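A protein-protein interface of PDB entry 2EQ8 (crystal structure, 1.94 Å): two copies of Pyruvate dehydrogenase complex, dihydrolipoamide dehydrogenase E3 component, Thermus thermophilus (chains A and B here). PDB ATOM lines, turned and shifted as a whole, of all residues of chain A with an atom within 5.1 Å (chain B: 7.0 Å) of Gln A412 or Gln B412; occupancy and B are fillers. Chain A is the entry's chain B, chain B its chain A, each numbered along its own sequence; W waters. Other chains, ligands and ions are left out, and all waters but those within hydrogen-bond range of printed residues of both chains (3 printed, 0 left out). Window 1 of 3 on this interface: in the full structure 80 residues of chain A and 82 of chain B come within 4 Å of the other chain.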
ATOM      1  N   GLU A 351      36.482  19.139  -2.675  1.00  0.00           N
ATOM      2  CA  GLU A 351      35.554  19.842  -1.806  1.00  0.00           C
ATOM      3  C   GLU A 351      35.119  18.889  -0.700  1.00  0.00           C
ATOM      4  O   GLU A 351      35.281  17.677  -0.817  1.00  0.00           O
ATOM      5  CB  GLU A 351      34.302  20.284  -2.575  1.00  0.00           C
ATOM      6  CG  GLU A 351      34.566  21.182  -3.768  1.00  0.00           C
ATOM      7  CD  GLU A 351      33.294  21.772  -4.360  1.00  0.00           C
ATOM      8  OE1 GLU A 351      32.179  21.354  -3.969  1.00  0.00           O
ATOM      9  OE2 GLU A 351      33.420  22.656  -5.227  1.00  0.00           O
ATOM     10  N   GLY A 410      35.290  15.247  -2.427  1.00  0.00           N
ATOM     11  CA  GLY A 410      35.603  15.032  -3.823  1.00  0.00           C
ATOM     12  C   GLY A 410      35.131  16.221  -4.639  1.00  0.00           C
ATOM     13  O   GLY A 410      34.590  17.178  -4.082  1.00  0.00           O
ATOM     14  N   PRO A 411      35.329  16.203  -5.958  1.00  0.00           N
ATOM     15  CA  PRO A 411      34.873  17.348  -6.749  1.00  0.00           C
ATOM     16  C   PRO A 411      33.350  17.477  -6.727  1.00  0.00           C
ATOM     17  O   PRO A 411      32.634  16.479  -6.673  1.00  0.00           O
ATOM     18  CB  PRO A 411      35.430  17.051  -8.143  1.00  0.00           C
ATOM     19  CG  PRO A 411      35.475  15.538  -8.175  1.00  0.00           C
ATOM     20  CD  PRO A 411      35.997  15.197  -6.801  1.00  0.00           C
ATOM     21  N   GLN A 412      32.868  18.715  -6.731  1.00  0.00           N
ATOM     22  CA  GLN A 412      31.435  18.998  -6.728  1.00  0.00           C
ATOM     23  C   GLN A 412      30.697  18.512  -5.482  1.00  0.00           C
ATOM     24  O   GLN A 412      29.473  18.428  -5.481  1.00  0.00           O
ATOM     25  CB  GLN A 412      30.787  18.387  -7.978  1.00  0.00           C
ATOM     26  CG  GLN A 412      31.489  18.765  -9.273  1.00  0.00           C
ATOM     27  CD  GLN A 412      31.509  20.266  -9.515  1.00  0.00           C
ATOM     28  OE1 GLN A 412      32.371  20.779 -10.232  1.00  0.00           O
ATOM     29  NE2 GLN A 412      30.552  20.972  -8.930  1.00  0.00           N
ATOM     30  N   ALA A 413      31.431  18.191  -4.421  1.00  0.00           N
ATOM     31  CA  ALA A 413      30.786  17.728  -3.189  1.00  0.00           C
ATOM     32  C   ALA A 413      29.695  18.714  -2.779  1.00  0.00           C
ATOM     33  O   ALA A 413      28.613  18.320  -2.341  1.00  0.00           O
ATOM     34  CB  ALA A 413      31.811  17.609  -2.073  1.00  0.00           C
ATOM     35  N   GLY A 414      30.000  20.001  -2.922  1.00  0.00           N
ATOM     36  CA  GLY A 414      29.054  21.041  -2.555  1.00  0.00           C
ATOM     37  C   GLY A 414      27.751  20.996  -3.327  1.00  0.00           C
ATOM     38  O   GLY A 414      26.701  21.384  -2.807  1.00  0.00           O
ATOM     39  N   GLU A 415      27.807  20.526  -4.569  1.00  0.00           N
ATOM     40  CA  GLU A 415      26.601  20.445  -5.397  1.00  0.00           C
ATOM     41  C   GLU A 415      25.799  19.185  -5.091  1.00  0.00           C
ATOM     42  O   GLU A 415      24.574  19.179  -5.180  1.00  0.00           O
ATOM     43  CB  GLU A 415      26.982  20.456  -6.881  1.00  0.00           C
ATOM     44  CG  GLU A 415      27.749  21.693  -7.315  1.00  0.00           C
ATOM     45  CD  GLU A 415      26.876  22.934  -7.365  1.00  0.00           C
ATOM     46  OE1 GLU A 415      27.400  24.019  -7.697  1.00  0.00           O
ATOM     47  OE2 GLU A 415      25.665  22.825  -7.077  1.00  0.00           O
ATOM     48  N   LEU A 416      26.500  18.121  -4.714  1.00  0.00           N
ATOM     49  CA  LEU A 416      25.866  16.839  -4.429  1.00  0.00           C
ATOM     50  C   LEU A 416      25.167  16.750  -3.077  1.00  0.00           C
ATOM     51  O   LEU A 416      24.235  15.963  -2.904  1.00  0.00           O
ATOM     52  CB  LEU A 416      26.909  15.725  -4.525  1.00  0.00           C
ATOM     53  CG  LEU A 416      27.754  15.687  -5.804  1.00  0.00           C
ATOM     54  CD1 LEU A 416      28.783  14.562  -5.704  1.00  0.00           C
ATOM     55  CD2 LEU A 416      26.852  15.493  -7.024  1.00  0.00           C
ATOM     56  N   LEU A 443      29.278  12.094 -10.896  1.00  0.00           N
ATOM     57  CA  LEU A 443      29.824  12.005  -9.554  1.00  0.00           C
ATOM     58  C   LEU A 443      28.700  11.684  -8.566  1.00  0.00           C
ATOM     59  O   LEU A 443      28.939  11.047  -7.534  1.00  0.00           O
ATOM     60  CB  LEU A 443      30.504  13.321  -9.176  1.00  0.00           C
ATOM     61  CG  LEU A 443      31.688  13.731 -10.061  1.00  0.00           C
ATOM     62  CD1 LEU A 443      32.091  15.172  -9.754  1.00  0.00           C
ATOM     63  CD2 LEU A 443      32.863  12.783  -9.838  1.00  0.00           C
ATOM     64  N   THR B 348      27.499  18.366 -23.007  1.00  0.00           N
ATOM     65  CA  THR B 348      28.051  19.502 -23.726  1.00  0.00           C
ATOM     66  C   THR B 348      28.293  20.565 -22.659  1.00  0.00           C
ATOM     67  O   THR B 348      27.989  20.362 -21.487  1.00  0.00           O
ATOM     68  CB  THR B 348      27.026  20.083 -24.708  1.00  0.00           C
ATOM     69  OG1 THR B 348      25.748  20.142 -24.062  1.00  0.00           O
ATOM     70  CG2 THR B 348      26.923  19.238 -25.961  1.00  0.00           C
ATOM     71  N   PRO B 350      27.297  24.514 -22.164  1.00  0.00           N
ATOM     72  CA  PRO B 350      26.668  24.060 -20.918  1.00  0.00           C
ATOM     73  C   PRO B 350      26.048  22.670 -21.043  1.00  0.00           C
ATOM     74  O   PRO B 350      25.755  22.208 -22.147  1.00  0.00           O
ATOM     75  CB  PRO B 350      25.615  25.132 -20.668  1.00  0.00           C
ATOM     76  CG  PRO B 350      25.169  25.461 -22.058  1.00  0.00           C
ATOM     77  CD  PRO B 350      26.495  25.589 -22.782  1.00  0.00           C
ATOM     78  N   GLU B 351      25.847  21.998 -19.917  1.00  0.00           N
ATOM     79  CA  GLU B 351      25.247  20.671 -19.962  1.00  0.00           C
ATOM     80  C   GLU B 351      23.737  20.808 -20.019  1.00  0.00           C
ATOM     81  O   GLU B 351      23.187  21.864 -19.700  1.00  0.00           O
ATOM     82  CB  GLU B 351      25.603  19.846 -18.716  1.00  0.00           C
ATOM     83  CG  GLU B 351      27.080  19.730 -18.415  1.00  0.00           C
ATOM     84  CD  GLU B 351      27.373  18.654 -17.378  1.00  0.00           C
ATOM     85  OE1 GLU B 351      26.470  18.310 -16.582  1.00  0.00           O
ATOM     86  OE2 GLU B 351      28.515  18.159 -17.354  1.00  0.00           O
ATOM     87  N   ALA B 353      20.114  18.566 -18.940  1.00  0.00           N
ATOM     88  CA  ALA B 353      19.612  17.416 -18.191  1.00  0.00           C
ATOM     89  C   ALA B 353      18.123  17.557 -17.948  1.00  0.00           C
ATOM     90  O   ALA B 353      17.607  18.667 -17.775  1.00  0.00           O
ATOM     91  CB  ALA B 353      20.343  17.284 -16.859  1.00  0.00           C
ATOM     92  N   ARG B 381      27.043  31.739  -7.634  1.00  0.00           N
ATOM     93  CA  ARG B 381      28.012  30.675  -7.884  1.00  0.00           C
ATOM     94  C   ARG B 381      28.413  30.657  -9.359  1.00  0.00           C
ATOM     95  O   ARG B 381      29.594  30.551  -9.692  1.00  0.00           O
ATOM     96  CB  ARG B 381      27.437  29.310  -7.489  1.00  0.00           C
ATOM     97  CG  ARG B 381      28.429  28.143  -7.622  1.00  0.00           C
ATOM     98  CD  ARG B 381      29.801  28.488  -7.016  1.00  0.00           C
ATOM     99  NE  ARG B 381      30.694  27.330  -6.944  1.00  0.00           N
ATOM    100  CZ  ARG B 381      32.023  27.408  -6.915  1.00  0.00           C
ATOM    101  NH1 ARG B 381      32.624  28.591  -6.957  1.00  0.00           N
ATOM    102  NH2 ARG B 381      32.756  26.304  -6.834  1.00  0.00           N
ATOM    103  N   LEU B 385      32.237  31.144 -11.230  1.00  0.00           N
ATOM    104  CA  LEU B 385      32.784  30.102 -12.088  1.00  0.00           C
ATOM    105  C   LEU B 385      33.147  30.693 -13.455  1.00  0.00           C
ATOM    106  O   LEU B 385      33.467  29.971 -14.403  1.00  0.00           O
ATOM    107  CB  LEU B 385      31.785  28.948 -12.236  1.00  0.00           C
ATOM    108  CG  LEU B 385      31.497  28.165 -10.940  1.00  0.00           C
ATOM    109  CD1 LEU B 385      30.437  27.098 -11.190  1.00  0.00           C
ATOM    110  CD2 LEU B 385      32.776  27.526 -10.433  1.00  0.00           C
ATOM    111  N   ILE B 408      17.195  21.236 -16.836  1.00  0.00           N
ATOM    112  CA  ILE B 408      18.305  22.114 -16.532  1.00  0.00           C
ATOM    113  C   ILE B 408      19.286  22.288 -17.682  1.00  0.00           C
ATOM    114  O   ILE B 408      19.627  21.336 -18.381  1.00  0.00           O
ATOM    115  CB  ILE B 408      19.103  21.547 -15.331  1.00  0.00           C
ATOM    116  CG1 ILE B 408      18.143  21.176 -14.200  1.00  0.00           C
ATOM    117  CG2 ILE B 408      20.150  22.555 -14.867  1.00  0.00           C
ATOM    118  CD1 ILE B 408      18.788  20.393 -13.065  1.00  0.00           C
ATOM    119  N   GLY B 410      23.008  24.239 -18.196  1.00  0.00           N
ATOM    120  CA  GLY B 410      24.060  24.988 -17.538  1.00  0.00           C
ATOM    121  C   GLY B 410      25.156  24.071 -17.031  1.00  0.00           C
ATOM    122  O   GLY B 410      25.083  22.857 -17.223  1.00  0.00           O
ATOM    123  N   PRO B 411      26.193  24.617 -16.382  1.00  0.00           N
ATOM    124  CA  PRO B 411      27.271  23.765 -15.874  1.00  0.00           C
ATOM    125  C   PRO B 411      26.778  22.826 -14.776  1.00  0.00           C
ATOM    126  O   PRO B 411      25.928  23.199 -13.968  1.00  0.00           O
ATOM    127  CB  PRO B 411      28.299  24.775 -15.364  1.00  0.00           C
ATOM    128  CG  PRO B 411      27.445  25.934 -14.938  1.00  0.00           C
ATOM    129  CD  PRO B 411      26.439  26.034 -16.059  1.00  0.00           C
ATOM    130  N   GLN B 412      27.304  21.603 -14.776  1.00  0.00           N
ATOM    131  CA  GLN B 412      26.950  20.584 -13.788  1.00  0.00           C
ATOM    132  C   GLN B 412      25.477  20.151 -13.812  1.00  0.00           C
ATOM    133  O   GLN B 412      24.987  19.531 -12.863  1.00  0.00           O
ATOM    134  CB  GLN B 412      27.322  21.079 -12.381  1.00  0.00           C
ATOM    135  CG  GLN B 412      28.765  21.567 -12.262  1.00  0.00           C
ATOM    136  CD  GLN B 412      29.785  20.491 -12.602  1.00  0.00           C
ATOM    137  OE1 GLN B 412      30.899  20.791 -13.043  1.00  0.00           O
ATOM    138  NE2 GLN B 412      29.418  19.236 -12.386  1.00  0.00           N
ATOM    139  N   ALA B 413      24.773  20.457 -14.897  1.00  0.00           N
ATOM    140  CA  ALA B 413      23.365  20.078 -14.996  1.00  0.00           C
ATOM    141  C   ALA B 413      23.161  18.586 -14.741  1.00  0.00           C
ATOM    142  O   ALA B 413      22.167  18.187 -14.132  1.00  0.00           O
ATOM    143  CB  ALA B 413      22.816  20.441 -16.372  1.00  0.00           C
ATOM    144  N   GLY B 414      24.107  17.773 -15.211  1.00  0.00           N
ATOM    145  CA  GLY B 414      24.015  16.331 -15.049  1.00  0.00           C
ATOM    146  C   GLY B 414      24.125  15.855 -13.617  1.00  0.00           C
ATOM    147  O   GLY B 414      23.617  14.785 -13.264  1.00  0.00           O
ATOM    148  N   GLU B 415      24.792  16.649 -12.788  1.00  0.00           N
ATOM    149  CA  GLU B 415      24.967  16.313 -11.384  1.00  0.00           C
ATOM    150  C   GLU B 415      23.750  16.788 -10.601  1.00  0.00           C
ATOM    151  O   GLU B 415      23.301  16.118  -9.677  1.00  0.00           O
ATOM    152  CB  GLU B 415      26.229  16.980 -10.834  1.00  0.00           C
ATOM    153  CG  GLU B 415      27.516  16.561 -11.531  1.00  0.00           C
ATOM    154  CD  GLU B 415      27.881  15.105 -11.283  1.00  0.00           C
ATOM    155  OE1 GLU B 415      28.876  14.635 -11.878  1.00  0.00           O
ATOM    156  OE2 GLU B 415      27.179  14.432 -10.490  1.00  0.00           O
ATOM    157  N   LEU B 416      23.215  17.940 -10.987  1.00  0.00           N
ATOM    158  CA  LEU B 416      22.058  18.510 -10.310  1.00  0.00           C
ATOM    159  C   LEU B 416      20.770  17.738 -10.568  1.00  0.00           C
ATOM    160  O   LEU B 416      19.873  17.722  -9.726  1.00  0.00           O
ATOM    161  CB  LEU B 416      21.863  19.968 -10.738  1.00  0.00           C
ATOM    162  CG  LEU B 416      23.073  20.902 -10.604  1.00  0.00           C
ATOM    163  CD1 LEU B 416      22.687  22.288 -11.107  1.00  0.00           C
ATOM    164  CD2 LEU B 416      23.547  20.967  -9.156  1.00  0.00           C
ATOM    165  N   ILE B 417      20.676  17.091 -11.725  1.00  0.00           N
ATOM    166  CA  ILE B 417      19.472  16.352 -12.063  1.00  0.00           C
ATOM    167  C   ILE B 417      19.210  15.179 -11.102  1.00  0.00           C
ATOM    168  O   ILE B 417      18.063  14.765 -10.922  1.00  0.00           O
ATOM    169  CB  ILE B 417      19.521  15.873 -13.545  1.00  0.00           C
ATOM    170  CG1 ILE B 417      18.096  15.710 -14.079  1.00  0.00           C
ATOM    171  CG2 ILE B 417      20.304  14.574 -13.671  1.00  0.00           C
ATOM    172  CD1 ILE B 417      17.316  17.017 -14.146  1.00  0.00           C
ATOM    173  N   LEU B 443      25.366  25.892  -7.561  1.00  0.00           N
ATOM    174  CA  LEU B 443      24.498  25.875  -8.727  1.00  0.00           C
ATOM    175  C   LEU B 443      23.186  25.164  -8.363  1.00  0.00           C
ATOM    176  O   LEU B 443      22.131  25.461  -8.932  1.00  0.00           O
ATOM    177  CB  LEU B 443      25.201  25.156  -9.885  1.00  0.00           C
ATOM    178  CG  LEU B 443      26.536  25.779 -10.328  1.00  0.00           C
ATOM    179  CD1 LEU B 443      27.271  24.838 -11.265  1.00  0.00           C
ATOM    180  CD2 LEU B 443      26.276  27.119 -11.009  1.00  0.00           C
HETATM  181  O   HOH W   1      35.190  24.412  -5.273  1.00  0.00           O
HETATM  182  O   HOH W   2      29.365  24.979  -6.281  1.00  0.00           O
HETATM  183  O   HOH W   3      32.082  23.620  -6.980  1.00  0.00           O
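OE1 of Glu A415 is in hydrogen-bond range of N of Leu B443, at 2.8 Å. OE1 of Gln B412 lies close to OE1 of Gln A412 (3.2 Å). The side-chain carboxylate (OE1) of Glu B415 is in hydrogen-bond range of the backbone NH (N) of Leu A443 (2.8 Å).
Leu B416 touches Glu A415 (CD2 to OE2, 3.5 Å). OE2 of Glu B415 touches CD2 of Leu A416, at 3.6 Å.
Printed residues of chain B within 4 Å of Gln A412: Gln B412 (3.2 Å). Gln B412 touches one residue of chain A. Of the printed residues of chain A, Leu B416 touches Glu A415. Printed residues of chain A within 4 Å of Glu B415: Leu A416 and Leu A443. Of the printed residues of chain B, Leu A416 touches Glu B415. Gly B414 touches none of the printed residues of chain A. The nearest printed residue of chain B that does not touch Leu A443 is Gln B412 (5.5 Å).
Hydrophobic or aromatic side chains of chain B that line the printed part of chain A: Leu B416 and Leu B443.
Gln A412 touches its own counterpart, Gln B412. Glu A415 touches Leu B416, and with the chains exchanged Leu A416 touches Glu B415. Glu A415 touches Leu B443, and with the chains exchanged Leu A443 touches Glu B415. 9 positions are printed for both chains.
Water W3 bridges the side-chain carboxylate (OE2) of Glu A351 (2.4 Å) and the guanidinium group (NH2) of Arg B381 (2.8 Å). Water W1 bridges OE2 of Glu A351 and NH2 of Arg B381. Water W2 lies within hydrogen-bond range of the side-chain carboxylate (OE1) of Glu A415 and the guanidinium group (NE) of Arg B381.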
